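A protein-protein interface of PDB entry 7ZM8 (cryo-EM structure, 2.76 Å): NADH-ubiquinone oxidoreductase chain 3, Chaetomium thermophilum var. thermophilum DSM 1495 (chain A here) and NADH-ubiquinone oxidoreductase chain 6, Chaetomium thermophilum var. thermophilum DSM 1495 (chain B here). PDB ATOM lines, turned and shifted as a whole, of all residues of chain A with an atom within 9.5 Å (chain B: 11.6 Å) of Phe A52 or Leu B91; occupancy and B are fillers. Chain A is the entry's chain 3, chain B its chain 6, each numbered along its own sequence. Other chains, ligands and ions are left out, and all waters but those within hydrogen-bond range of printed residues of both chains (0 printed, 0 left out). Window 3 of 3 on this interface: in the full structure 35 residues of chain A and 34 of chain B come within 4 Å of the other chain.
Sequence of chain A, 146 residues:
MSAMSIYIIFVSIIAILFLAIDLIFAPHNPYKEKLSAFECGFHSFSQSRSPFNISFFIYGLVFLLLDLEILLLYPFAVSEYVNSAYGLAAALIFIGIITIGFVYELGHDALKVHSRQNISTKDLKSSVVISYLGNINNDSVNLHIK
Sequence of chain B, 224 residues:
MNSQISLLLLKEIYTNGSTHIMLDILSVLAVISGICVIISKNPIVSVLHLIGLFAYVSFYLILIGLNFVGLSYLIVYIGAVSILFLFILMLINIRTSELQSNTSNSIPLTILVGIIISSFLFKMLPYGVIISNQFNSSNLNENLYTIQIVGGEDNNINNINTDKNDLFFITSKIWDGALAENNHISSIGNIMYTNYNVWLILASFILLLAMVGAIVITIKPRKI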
ATOM      1  N   SER A  48      -7.590  11.556 -19.526  1.00  0.00           N
ATOM      2  CA  SER A  48      -8.245  11.343 -18.243  1.00  0.00           C
ATOM      3  C   SER A  48      -9.218  10.185 -18.390  1.00  0.00           C
ATOM      4  O   SER A  48      -9.588   9.798 -19.502  1.00  0.00           O
ATOM      5  CB  SER A  48      -8.969  12.605 -17.760  1.00  0.00           C
ATOM      6  OG  SER A  48      -9.861  13.090 -18.747  1.00  0.00           O
ATOM      7  N   ARG A  49      -9.626   9.633 -17.252  1.00  0.00           N
ATOM      8  CA  ARG A  49     -10.530   8.493 -17.226  1.00  0.00           C
ATOM      9  C   ARG A  49     -11.676   8.758 -16.267  1.00  0.00           C
ATOM     10  O   ARG A  49     -11.465   9.218 -15.142  1.00  0.00           O
ATOM     11  CB  ARG A  49      -9.802   7.214 -16.816  1.00  0.00           C
ATOM     12  CG  ARG A  49      -8.673   6.823 -17.748  1.00  0.00           C
ATOM     13  CD  ARG A  49      -8.218   5.412 -17.458  1.00  0.00           C
ATOM     14  NE  ARG A  49      -9.347   4.493 -17.506  1.00  0.00           N
ATOM     15  CZ  ARG A  49      -9.258   3.182 -17.317  1.00  0.00           C
ATOM     16  NH1 ARG A  49      -8.084   2.621 -17.070  1.00  0.00           N
ATOM     17  NH2 ARG A  49     -10.348   2.434 -17.384  1.00  0.00           N
ATOM     18  N   SER A  50     -12.891   8.460 -16.721  1.00  0.00           N
ATOM     19  CA  SER A  50     -14.084   8.565 -15.894  1.00  0.00           C
ATOM     20  C   SER A  50     -15.100   7.571 -16.416  1.00  0.00           C
ATOM     21  O   SER A  50     -15.159   7.334 -17.627  1.00  0.00           O
ATOM     22  CB  SER A  50     -14.662   9.985 -15.918  1.00  0.00           C
ATOM     23  OG  SER A  50     -13.853  10.874 -15.170  1.00  0.00           O
ATOM     24  N   PRO A  51     -15.894   6.965 -15.543  1.00  0.00           N
ATOM     25  CA  PRO A  51     -16.904   6.014 -16.008  1.00  0.00           C
ATOM     26  C   PRO A  51     -17.964   6.701 -16.847  1.00  0.00           C
ATOM     27  O   PRO A  51     -18.331   7.852 -16.607  1.00  0.00           O
ATOM     28  CB  PRO A  51     -17.500   5.459 -14.708  1.00  0.00           C
ATOM     29  CG  PRO A  51     -16.624   5.950 -13.612  1.00  0.00           C
ATOM     30  CD  PRO A  51     -15.976   7.191 -14.094  1.00  0.00           C
ATOM     31  N   PHE A  52     -18.466   5.976 -17.837  1.00  0.00           N
ATOM     32  CA  PHE A  52     -19.557   6.458 -18.665  1.00  0.00           C
ATOM     33  C   PHE A  52     -20.878   5.891 -18.165  1.00  0.00           C
ATOM     34  O   PHE A  52     -20.934   4.798 -17.596  1.00  0.00           O
ATOM     35  CB  PHE A  52     -19.341   6.091 -20.138  1.00  0.00           C
ATOM     36  CG  PHE A  52     -19.505   4.629 -20.440  1.00  0.00           C
ATOM     37  CD1 PHE A  52     -18.453   3.756 -20.273  1.00  0.00           C
ATOM     38  CD2 PHE A  52     -20.705   4.137 -20.919  1.00  0.00           C
ATOM     39  CE1 PHE A  52     -18.598   2.425 -20.559  1.00  0.00           C
ATOM     40  CE2 PHE A  52     -20.857   2.801 -21.204  1.00  0.00           C
ATOM     41  CZ  PHE A  52     -19.802   1.944 -21.024  1.00  0.00           C
ATOM     42  N   ASN A  53     -21.944   6.655 -18.376  1.00  0.00           N
ATOM     43  CA  ASN A  53     -23.260   6.250 -17.907  1.00  0.00           C
ATOM     44  C   ASN A  53     -23.778   5.059 -18.698  1.00  0.00           C
ATOM     45  O   ASN A  53     -23.664   5.010 -19.925  1.00  0.00           O
ATOM     46  CB  ASN A  53     -24.237   7.413 -18.014  1.00  0.00           C
ATOM     47  CG  ASN A  53     -23.787   8.619 -17.223  1.00  0.00           C
ATOM     48  OD1 ASN A  53     -23.764   8.596 -15.992  1.00  0.00           O
ATOM     49  ND2 ASN A  53     -23.416   9.684 -17.925  1.00  0.00           N
ATOM     50  N   ILE A  54     -24.361   4.096 -17.982  1.00  0.00           N
ATOM     51  CA  ILE A  54     -24.952   2.936 -18.629  1.00  0.00           C
ATOM     52  C   ILE A  54     -26.147   3.325 -19.487  1.00  0.00           C
ATOM     53  O   ILE A  54     -26.569   2.549 -20.347  1.00  0.00           O
ATOM     54  CB  ILE A  54     -25.326   1.887 -17.563  1.00  0.00           C
ATOM     55  CG1 ILE A  54     -25.671   0.548 -18.215  1.00  0.00           C
ATOM     56  CG2 ILE A  54     -26.487   2.380 -16.722  1.00  0.00           C
ATOM     57  CD1 ILE A  54     -24.539  -0.054 -18.975  1.00  0.00           C
ATOM     58  N   SER A  55     -26.644   4.530 -19.307  1.00  0.00           N
ATOM     59  CA  SER A  55     -27.854   4.972 -20.027  1.00  0.00           C
ATOM     60  C   SER A  55     -27.579   5.015 -21.525  1.00  0.00           C
ATOM     61  O   SER A  55     -28.469   4.614 -22.283  1.00  0.00           O
ATOM     62  CB  SER A  55     -28.292   6.294 -19.473  1.00  0.00           C
ATOM     63  OG  SER A  55     -27.286   7.277 -19.663  1.00  0.00           O
ATOM     64  N   PHE A  56     -26.392   5.474 -21.919  1.00  0.00           N
ATOM     65  CA  PHE A  56     -26.004   5.551 -23.353  1.00  0.00           C
ATOM     66  C   PHE A  56     -26.125   4.180 -24.021  1.00  0.00           C
ATOM     67  O   PHE A  56     -26.576   4.119 -25.175  1.00  0.00           O
ATOM     68  CB  PHE A  56     -24.602   6.143 -23.491  1.00  0.00           C
ATOM     69  CG  PHE A  56     -24.533   7.629 -23.256  1.00  0.00           C
ATOM     70  CD1 PHE A  56     -25.200   8.507 -24.094  1.00  0.00           C
ATOM     71  CD2 PHE A  56     -23.799   8.149 -22.204  1.00  0.00           C
ATOM     72  CE1 PHE A  56     -25.137   9.874 -23.881  1.00  0.00           C
ATOM     73  CE2 PHE A  56     -23.736   9.517 -21.992  1.00  0.00           C
ATOM     74  CZ  PHE A  56     -24.403  10.376 -22.833  1.00  0.00           C
ATOM     75  N   PHE A  57     -25.724   3.120 -23.320  1.00  0.00           N
ATOM     76  CA  PHE A  57     -25.875   1.784 -23.880  1.00  0.00           C
ATOM     77  C   PHE A  57     -27.343   1.426 -24.052  1.00  0.00           C
ATOM     78  O   PHE A  57     -27.732   0.843 -25.069  1.00  0.00           O
ATOM     79  CB  PHE A  57     -25.170   0.753 -22.999  1.00  0.00           C
ATOM     80  CG  PHE A  57     -25.456  -0.660 -23.395  1.00  0.00           C
ATOM     81  CD1 PHE A  57     -25.044  -1.145 -24.620  1.00  0.00           C
ATOM     82  CD2 PHE A  57     -26.173  -1.493 -22.563  1.00  0.00           C
ATOM     83  CE1 PHE A  57     -25.329  -2.438 -24.998  1.00  0.00           C
ATOM     84  CE2 PHE A  57     -26.458  -2.782 -22.935  1.00  0.00           C
ATOM     85  CZ  PHE A  57     -26.038  -3.254 -24.154  1.00  0.00           C
ATOM     86  N   ILE A  58     -28.170   1.769 -23.067  1.00  0.00           N
ATOM     87  CA  ILE A  58     -29.567   1.353 -23.072  1.00  0.00           C
ATOM     88  C   ILE A  58     -30.333   2.036 -24.196  1.00  0.00           C
ATOM     89  O   ILE A  58     -31.236   1.445 -24.795  1.00  0.00           O
ATOM     90  CB  ILE A  58     -30.197   1.632 -21.697  1.00  0.00           C
ATOM     91  CG1 ILE A  58     -29.309   1.067 -20.586  1.00  0.00           C
ATOM     92  CG2 ILE A  58     -31.608   1.067 -21.623  1.00  0.00           C
ATOM     93  CD1 ILE A  58     -28.978  -0.378 -20.743  1.00  0.00           C
ATOM     94  N   TYR A  59     -29.995   3.289 -24.498  1.00  0.00           N
ATOM     95  CA  TYR A  59     -30.691   4.005 -25.560  1.00  0.00           C
ATOM     96  C   TYR A  59     -30.494   3.320 -26.905  1.00  0.00           C
ATOM     97  O   TYR A  59     -31.442   3.162 -27.679  1.00  0.00           O
ATOM     98  CB  TYR A  59     -30.215   5.455 -25.611  1.00  0.00           C
ATOM     99  CG  TYR A  59     -30.708   6.271 -24.446  1.00  0.00           C
ATOM    100  CD1 TYR A  59     -31.965   6.057 -23.918  1.00  0.00           C
ATOM    101  CD2 TYR A  59     -29.915   7.244 -23.865  1.00  0.00           C
ATOM    102  CE1 TYR A  59     -32.422   6.787 -22.849  1.00  0.00           C
ATOM    103  CE2 TYR A  59     -30.368   7.985 -22.794  1.00  0.00           C
ATOM    104  CZ  TYR A  59     -31.625   7.747 -22.292  1.00  0.00           C
ATOM    105  OH  TYR A  59     -32.098   8.474 -21.227  1.00  0.00           O
ATOM    106  N   ASN B  42      -7.118   1.726 -35.162  1.00  0.00           N
ATOM    107  CA  ASN B  42      -8.159   2.236 -34.283  1.00  0.00           C
ATOM    108  C   ASN B  42      -9.437   1.424 -34.456  1.00  0.00           C
ATOM    109  O   ASN B  42      -9.883   1.218 -35.586  1.00  0.00           O
ATOM    110  CB  ASN B  42      -8.426   3.700 -34.583  1.00  0.00           C
ATOM    111  CG  ASN B  42      -9.244   4.369 -33.516  1.00  0.00           C
ATOM    112  OD1 ASN B  42      -9.349   3.877 -32.399  1.00  0.00           O
ATOM    113  ND2 ASN B  42      -9.825   5.510 -33.851  1.00  0.00           N
ATOM    114  N   PRO B  43     -10.038   0.932 -33.370  1.00  0.00           N
ATOM    115  CA  PRO B  43     -11.350   0.286 -33.498  1.00  0.00           C
ATOM    116  C   PRO B  43     -12.425   1.207 -34.036  1.00  0.00           C
ATOM    117  O   PRO B  43     -13.393   0.726 -34.634  1.00  0.00           O
ATOM    118  CB  PRO B  43     -11.658  -0.162 -32.064  1.00  0.00           C
ATOM    119  CG  PRO B  43     -10.352  -0.252 -31.409  1.00  0.00           C
ATOM    120  CD  PRO B  43      -9.496   0.805 -32.010  1.00  0.00           C
ATOM    121  N   ILE B  44     -12.302   2.516 -33.814  1.00  0.00           N
ATOM    122  CA  ILE B  44     -13.249   3.470 -34.382  1.00  0.00           C
ATOM    123  C   ILE B  44     -13.186   3.443 -35.903  1.00  0.00           C
ATOM    124  O   ILE B  44     -14.214   3.386 -36.585  1.00  0.00           O
ATOM    125  CB  ILE B  44     -12.972   4.883 -33.840  1.00  0.00           C
ATOM    126  CG1 ILE B  44     -13.261   4.963 -32.344  1.00  0.00           C
ATOM    127  CG2 ILE B  44     -13.805   5.912 -34.582  1.00  0.00           C
ATOM    128  CD1 ILE B  44     -14.727   4.964 -32.023  1.00  0.00           C
ATOM    129  N   VAL B  47     -14.760   0.314 -37.414  1.00  0.00           N
ATOM    130  CA  VAL B  47     -16.216   0.362 -37.446  1.00  0.00           C
ATOM    131  C   VAL B  47     -16.706   1.301 -38.545  1.00  0.00           C
ATOM    132  O   VAL B  47     -17.715   1.031 -39.201  1.00  0.00           O
ATOM    133  CB  VAL B  47     -16.756   0.753 -36.058  1.00  0.00           C
ATOM    134  CG1 VAL B  47     -18.196   1.206 -36.142  1.00  0.00           C
ATOM    135  CG2 VAL B  47     -16.638  -0.422 -35.109  1.00  0.00           C
ATOM    136  N   SER B  82     -24.445  -0.175 -36.014  1.00  0.00           N
ATOM    137  CA  SER B  82     -23.161   0.511 -35.972  1.00  0.00           C
ATOM    138  C   SER B  82     -23.186   1.705 -35.027  1.00  0.00           C
ATOM    139  O   SER B  82     -22.148   2.063 -34.467  1.00  0.00           O
ATOM    140  CB  SER B  82     -22.756   0.939 -37.380  1.00  0.00           C
ATOM    141  OG  SER B  82     -23.692   1.843 -37.923  1.00  0.00           O
ATOM    142  N   ILE B  83     -24.350   2.327 -34.829  1.00  0.00           N
ATOM    143  CA  ILE B  83     -24.457   3.408 -33.852  1.00  0.00           C
ATOM    144  C   ILE B  83     -24.183   2.892 -32.449  1.00  0.00           C
ATOM    145  O   ILE B  83     -23.466   3.528 -31.669  1.00  0.00           O
ATOM    146  CB  ILE B  83     -25.831   4.094 -33.955  1.00  0.00           C
ATOM    147  CG1 ILE B  83     -25.951   4.846 -35.280  1.00  0.00           C
ATOM    148  CG2 ILE B  83     -26.063   5.021 -32.783  1.00  0.00           C
ATOM    149  CD1 ILE B  83     -24.944   5.960 -35.437  1.00  0.00           C
ATOM    150  N   LEU B  84     -24.736   1.731 -32.108  1.00  0.00           N
ATOM    151  CA  LEU B  84     -24.403   1.109 -30.833  1.00  0.00           C
ATOM    152  C   LEU B  84     -22.916   0.788 -30.746  1.00  0.00           C
ATOM    153  O   LEU B  84     -22.344   0.786 -29.652  1.00  0.00           O
ATOM    154  CB  LEU B  84     -25.250  -0.147 -30.638  1.00  0.00           C
ATOM    155  CG  LEU B  84     -25.493  -0.647 -29.214  1.00  0.00           C
ATOM    156  CD1 LEU B  84     -25.797   0.509 -28.282  1.00  0.00           C
ATOM    157  CD2 LEU B  84     -26.624  -1.648 -29.196  1.00  0.00           C
ATOM    158  N   PHE B  85     -22.275   0.518 -31.885  1.00  0.00           N
ATOM    159  CA  PHE B  85     -20.837   0.279 -31.891  1.00  0.00           C
ATOM    160  C   PHE B  85     -20.048   1.567 -31.696  1.00  0.00           C
ATOM    161  O   PHE B  85     -18.998   1.559 -31.047  1.00  0.00           O
ATOM    162  CB  PHE B  85     -20.421  -0.410 -33.189  1.00  0.00           C
ATOM    163  CG  PHE B  85     -20.317  -1.895 -33.071  1.00  0.00           C
ATOM    164  CD1 PHE B  85     -19.148  -2.483 -32.629  1.00  0.00           C
ATOM    165  CD2 PHE B  85     -21.387  -2.704 -33.387  1.00  0.00           C
ATOM    166  CE1 PHE B  85     -19.050  -3.846 -32.508  1.00  0.00           C
ATOM    167  CE2 PHE B  85     -21.293  -4.069 -33.267  1.00  0.00           C
ATOM    168  CZ  PHE B  85     -20.125  -4.641 -32.825  1.00  0.00           C
ATOM    169  N   LEU B  86     -20.519   2.681 -32.260  1.00  0.00           N
ATOM    170  CA  LEU B  86     -19.851   3.954 -32.005  1.00  0.00           C
ATOM    171  C   LEU B  86     -19.993   4.383 -30.549  1.00  0.00           C
ATOM    172  O   LEU B  86     -19.027   4.859 -29.951  1.00  0.00           O
ATOM    173  CB  LEU B  86     -20.368   5.053 -32.933  1.00  0.00           C
ATOM    174  CG  LEU B  86     -19.804   5.201 -34.351  1.00  0.00           C
ATOM    175  CD1 LEU B  86     -18.330   5.553 -34.296  1.00  0.00           C
ATOM    176  CD2 LEU B  86     -20.032   4.022 -35.235  1.00  0.00           C
ATOM    177  N   PHE B  87     -21.183   4.212 -29.985  1.00  0.00           N
ATOM    178  CA  PHE B  87     -21.410   4.566 -28.561  1.00  0.00           C
ATOM    179  C   PHE B  87     -20.363   3.871 -27.689  1.00  0.00           C
ATOM    180  O   PHE B  87     -19.592   4.584 -27.036  1.00  0.00           O
ATOM    181  CB  PHE B  87     -22.802   4.130 -28.095  1.00  0.00           C
ATOM    182  CG  PHE B  87     -23.928   5.070 -28.443  1.00  0.00           C
ATOM    183  CD1 PHE B  87     -23.673   6.361 -28.873  1.00  0.00           C
ATOM    184  CD2 PHE B  87     -25.248   4.668 -28.323  1.00  0.00           C
ATOM    185  CE1 PHE B  87     -24.712   7.225 -29.183  1.00  0.00           C
ATOM    186  CE2 PHE B  87     -26.287   5.533 -28.632  1.00  0.00           C
ATOM    187  CZ  PHE B  87     -26.016   6.811 -29.060  1.00  0.00           C
ATOM    188  N   ILE B  88     -20.288   2.535 -27.720  1.00  0.00           N
ATOM    189  CA  ILE B  88     -19.410   1.789 -26.827  1.00  0.00           C
ATOM    190  C   ILE B  88     -17.953   2.129 -27.104  1.00  0.00           C
ATOM    191  O   ILE B  88     -17.138   2.234 -26.183  1.00  0.00           O
ATOM    192  CB  ILE B  88     -19.690   0.281 -26.957  1.00  0.00           C
ATOM    193  CG1 ILE B  88     -21.146  -0.005 -26.606  1.00  0.00           C
ATOM    194  CG2 ILE B  88     -18.784  -0.516 -26.054  1.00  0.00           C
ATOM    195  CD1 ILE B  88     -21.537   0.469 -25.228  1.00  0.00           C
ATOM    196  N   LEU B  89     -17.607   2.328 -28.374  1.00  0.00           N
ATOM    197  CA  LEU B  89     -16.214   2.582 -28.715  1.00  0.00           C
ATOM    198  C   LEU B  89     -15.790   3.992 -28.333  1.00  0.00           C
ATOM    199  O   LEU B  89     -14.666   4.203 -27.867  1.00  0.00           O
ATOM    200  CB  LEU B  89     -15.995   2.339 -30.199  1.00  0.00           C
ATOM    201  CG  LEU B  89     -15.740   0.898 -30.614  1.00  0.00           C
ATOM    202  CD1 LEU B  89     -15.345   0.879 -32.056  1.00  0.00           C
ATOM    203  CD2 LEU B  89     -14.660   0.281 -29.762  1.00  0.00           C
ATOM    204  N   MET B  90     -16.682   4.961 -28.525  1.00  0.00           N
ATOM    205  CA  MET B  90     -16.345   6.389 -28.259  1.00  0.00           C
ATOM    206  C   MET B  90     -16.432   6.664 -26.757  1.00  0.00           C
ATOM    207  O   MET B  90     -16.206   7.811 -26.383  1.00  0.00           O
ATOM    208  CB  MET B  90     -17.298   7.333 -28.998  1.00  0.00           C
ATOM    209  CG  MET B  90     -17.105   7.347 -30.502  1.00  0.00           C
ATOM    210  SD  MET B  90     -18.535   7.990 -31.409  1.00  0.00           S
ATOM    211  CE  MET B  90     -18.560   9.693 -30.859  1.00  0.00           C
ATOM    212  N   LEU B  91     -16.639   5.638 -25.930  1.00  0.00           N
ATOM    213  CA  LEU B  91     -16.852   5.845 -24.471  1.00  0.00           C
ATOM    214  C   LEU B  91     -15.847   5.003 -23.699  1.00  0.00           C
ATOM    215  O   LEU B  91     -15.358   5.479 -22.665  1.00  0.00           O
ATOM    216  CB  LEU B  91     -18.279   5.437 -24.101  1.00  0.00           C
ATOM    217  CG  LEU B  91     -19.357   6.492 -24.328  1.00  0.00           C
ATOM    218  CD1 LEU B  91     -20.733   5.919 -24.031  1.00  0.00           C
ATOM    219  CD2 LEU B  91     -19.094   7.723 -23.479  1.00  0.00           C
ATOM    220  N   ILE B  92     -15.564   3.790 -24.174  1.00  0.00           N
ATOM    221  CA  ILE B  92     -14.530   2.998 -23.521  1.00  0.00           C
ATOM    222  C   ILE B  92     -13.164   3.650 -23.703  1.00  0.00           C
ATOM    223  O   ILE B  92     -12.853   4.230 -24.750  1.00  0.00           O
ATOM    224  CB  ILE B  92     -14.540   1.553 -24.055  1.00  0.00           C
ATOM    225  CG1 ILE B  92     -15.700   0.762 -23.445  1.00  0.00           C
ATOM    226  CG2 ILE B  92     -13.201   0.876 -23.874  1.00  0.00           C
ATOM    227  CD1 ILE B  92     -15.853  -0.626 -24.013  1.00  0.00           C
ATOM    228  N   ASN B  93     -12.347   3.576 -22.657  1.00  0.00           N
ATOM    229  CA  ASN B  93     -10.958   4.011 -22.734  1.00  0.00           C
ATOM    230  C   ASN B  93     -10.183   2.998 -23.559  1.00  0.00           C
ATOM    231  O   ASN B  93      -9.996   1.855 -23.136  1.00  0.00           O
ATOM    232  CB  ASN B  93     -10.366   4.154 -21.337  1.00  0.00           C
ATOM    233  CG  ASN B  93     -10.879   5.378 -20.614  1.00  0.00           C
ATOM    234  OD1 ASN B  93     -11.547   5.272 -19.587  1.00  0.00           O
ATOM    235  ND2 ASN B  93     -10.575   6.553 -21.153  1.00  0.00           N
ATOM    236  N   ILE B  94      -9.732   3.409 -24.737  1.00  0.00           N
ATOM    237  CA  ILE B  94      -8.992   2.546 -25.647  1.00  0.00           C
ATOM    238  C   ILE B  94      -7.604   3.133 -25.830  1.00  0.00           C
ATOM    239  O   ILE B  94      -7.458   4.277 -26.278  1.00  0.00           O
ATOM    240  CB  ILE B  94      -9.703   2.396 -27.000  1.00  0.00           C
ATOM    241  CG1 ILE B  94     -11.006   1.615 -26.844  1.00  0.00           C
ATOM    242  CG2 ILE B  94      -8.795   1.717 -28.001  1.00  0.00           C
ATOM    243  CD1 ILE B  94     -12.097   2.060 -27.774  1.00  0.00           C
ATOM    244  N   ARG B  95      -6.586   2.353 -25.491  1.00  0.00           N
ATOM    245  CA  ARG B  95      -5.211   2.683 -25.825  1.00  0.00           C
ATOM    246  C   ARG B  95      -4.835   1.892 -27.070  1.00  0.00           C
ATOM    247  O   ARG B  95      -4.869   0.658 -27.063  1.00  0.00           O
ATOM    248  CB  ARG B  95      -4.271   2.374 -24.663  1.00  0.00           C
ATOM    249  CG  ARG B  95      -4.243   3.469 -23.614  1.00  0.00           C
ATOM    250  CD  ARG B  95      -3.060   3.329 -22.679  1.00  0.00           C
ATOM    251  NE  ARG B  95      -3.479   2.905 -21.348  1.00  0.00           N
ATOM    252  CZ  ARG B  95      -3.650   3.730 -20.322  1.00  0.00           C
ATOM    253  NH1 ARG B  95      -4.035   3.259 -19.144  1.00  0.00           N
ATOM    254  NH2 ARG B  95      -3.440   5.030 -20.474  1.00  0.00           N
ATOM    255  N   ALA B 214     -30.042  -8.332 -21.683  1.00  0.00           N
ATOM    256  CA  ALA B 214     -29.015  -7.270 -21.783  1.00  0.00           C
ATOM    257  C   ALA B 214     -29.189  -6.285 -20.631  1.00  0.00           C
ATOM    258  O   ALA B 214     -28.173  -5.869 -20.070  1.00  0.00           O
ATOM    259  CB  ALA B 214     -29.041  -6.620 -23.141  1.00  0.00           C
ATOM    260  N   ILE B 217     -27.897  -7.853 -17.193  1.00  0.00           N
ATOM    261  CA  ILE B 217     -26.420  -7.954 -17.030  1.00  0.00           C
ATOM    262  C   ILE B 217     -25.780  -6.575 -16.880  1.00  0.00           C
ATOM    263  O   ILE B 217     -24.687  -6.506 -16.344  1.00  0.00           O
ATOM    264  CB  ILE B 217     -25.785  -8.798 -18.151  1.00  0.00           C
ATOM    265  CG1 ILE B 217     -25.876  -8.107 -19.512  1.00  0.00           C
ATOM    266  CG2 ILE B 217     -26.360 -10.206 -18.156  1.00  0.00           C
ATOM    267  CD1 ILE B 217     -25.259  -8.881 -20.641  1.00  0.00           C
ATOM    268  N   THR B 218     -26.442  -5.511 -17.312  1.00  0.00           N
ATOM    269  CA  THR B 218     -25.797  -4.163 -17.277  1.00  0.00           C
ATOM    270  C   THR B 218     -26.296  -3.195 -16.195  1.00  0.00           C
ATOM    271  O   THR B 218     -25.455  -2.548 -15.591  1.00  0.00           O
ATOM    272  CB  THR B 218     -25.749  -3.533 -18.684  1.00  0.00           C
ATOM    273  OG1 THR B 218     -27.079  -3.511 -19.200  1.00  0.00           O
ATOM    274  CG2 THR B 218     -24.829  -4.249 -19.645  1.00  0.00           C
ATOM    275  N   ILE B 219     -27.591  -3.064 -15.984  1.00  0.00           N
ATOM    276  CA  ILE B 219     -28.138  -2.013 -15.072  1.00  0.00           C
ATOM    277  C   ILE B 219     -28.096  -2.403 -13.599  1.00  0.00           C
ATOM    278  O   ILE B 219     -28.094  -3.594 -13.298  1.00  0.00           O
ATOM    279  CB  ILE B 219     -29.541  -1.546 -15.521  1.00  0.00           C
ATOM    280  CG1 ILE B 219     -30.660  -2.408 -14.935  1.00  0.00           C
ATOM    281  CG2 ILE B 219     -29.627  -1.444 -17.035  1.00  0.00           C
ATOM    282  CD1 ILE B 219     -31.998  -1.715 -14.894  1.00  0.00           C
ATOM    283  N   LYS B 220     -28.049  -1.402 -12.728  1.00  0.00           N
ATOM    284  CA  LYS B 220     -28.104  -1.664 -11.279  1.00  0.00           C
ATOM    285  C   LYS B 220     -29.584  -1.685 -10.936  1.00  0.00           C
ATOM    286  O   LYS B 220     -30.267  -0.702 -11.245  1.00  0.00           O
ATOM    287  CB  LYS B 220     -27.420  -0.532 -10.514  1.00  0.00           C
ATOM    288  CG  LYS B 220     -27.349  -0.693  -9.002  1.00  0.00           C
ATOM    289  CD  LYS B 220     -26.417  -1.796  -8.560  1.00  0.00           C
ATOM    290  CE  LYS B 220     -26.397  -1.983  -7.060  1.00  0.00           C
ATOM    291  NZ  LYS B 220     -25.950  -0.755  -6.362  1.00  0.00           N
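Leu B91 touches two residues of chain A.
No residue of chain B comes within 4 Å of Ser A50.
No residue of chain B comes within 4 Å of Pro A51.
No residue of chain B comes within 4 Å of Asn A53.
Ile A54 touches just one residue of chain B: Thr B218.
Of chain B, only Phe B87 (3.5 Å) and Leu B91 (3.9 Å) come within 4 Å of Phe A56.
Of the printed residues of chain A, Thr B218 touches Ile A54, Phe A57 and Ile A58.
Of the printed residues of chain A, Leu B84 touches Phe A57 (3.8 Å).
Printed residues of chain A within 4 Å of Ile B219: Ile A58 (3.9 Å).
Of the printed residues of chain B, Ser A48 touches Asn B93 (3.8 Å).
Of the printed residues of chain A, Asn B93 touches Ser A48 and Arg A49.
Val B47 touches none of the printed residues of chain A.
Leu B89 touches none of the printed residues of chain A.
The nearest printed residue of chain B that does not touch Arg A49 is Arg B95 (4.6 Å).
Among the printed residues, merely in contact across the chains: Phe A56 with Phe B87 (3.5 Å), Phe A52 with Leu B91 (3.6 Å), Ile A54 with Thr B218 (3.7 Å), Phe A57 with Leu B84 (3.8 Å), Ser A48 with Asn B93 (3.8 Å), Phe A57 with Thr B218 (3.9 Å), Phe A57 with Ile B88 (3.9 Å), Ile A58 with Ile B219 (3.9 Å), Phe A56 with Leu B91 (3.9 Å) and Ile A58 with Thr B218 (3.98 Å).
OD1 of Asn B93 is in hydrogen-bond range of NE of Arg A49 (3.1 Å).
The backbone carbonyl oxygen (O) of Ala B214 is in hydrogen-bond range of the side-chain hydroxyl (OG1) of Thr B218, 2.7 Å away.
Printed residues of chain A that touch a printed residue of chain B: Ser A48, Arg A49, Phe A52, Ile A54, Phe A56, Phe A57 and Ile A58.
Hydrophobic or aromatic side chains of chain A that line the printed part of chain B: Phe A52, Ile A54, Phe A56, Phe A57 and Ile A58.
Of the 23 printed residues of chain B, 7 touch a printed residue of chain A.
Among the printed residues, no Asp or Glu carboxylate lies within 4 Å of a Lys or Arg side-chain nitrogen of the other chain.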
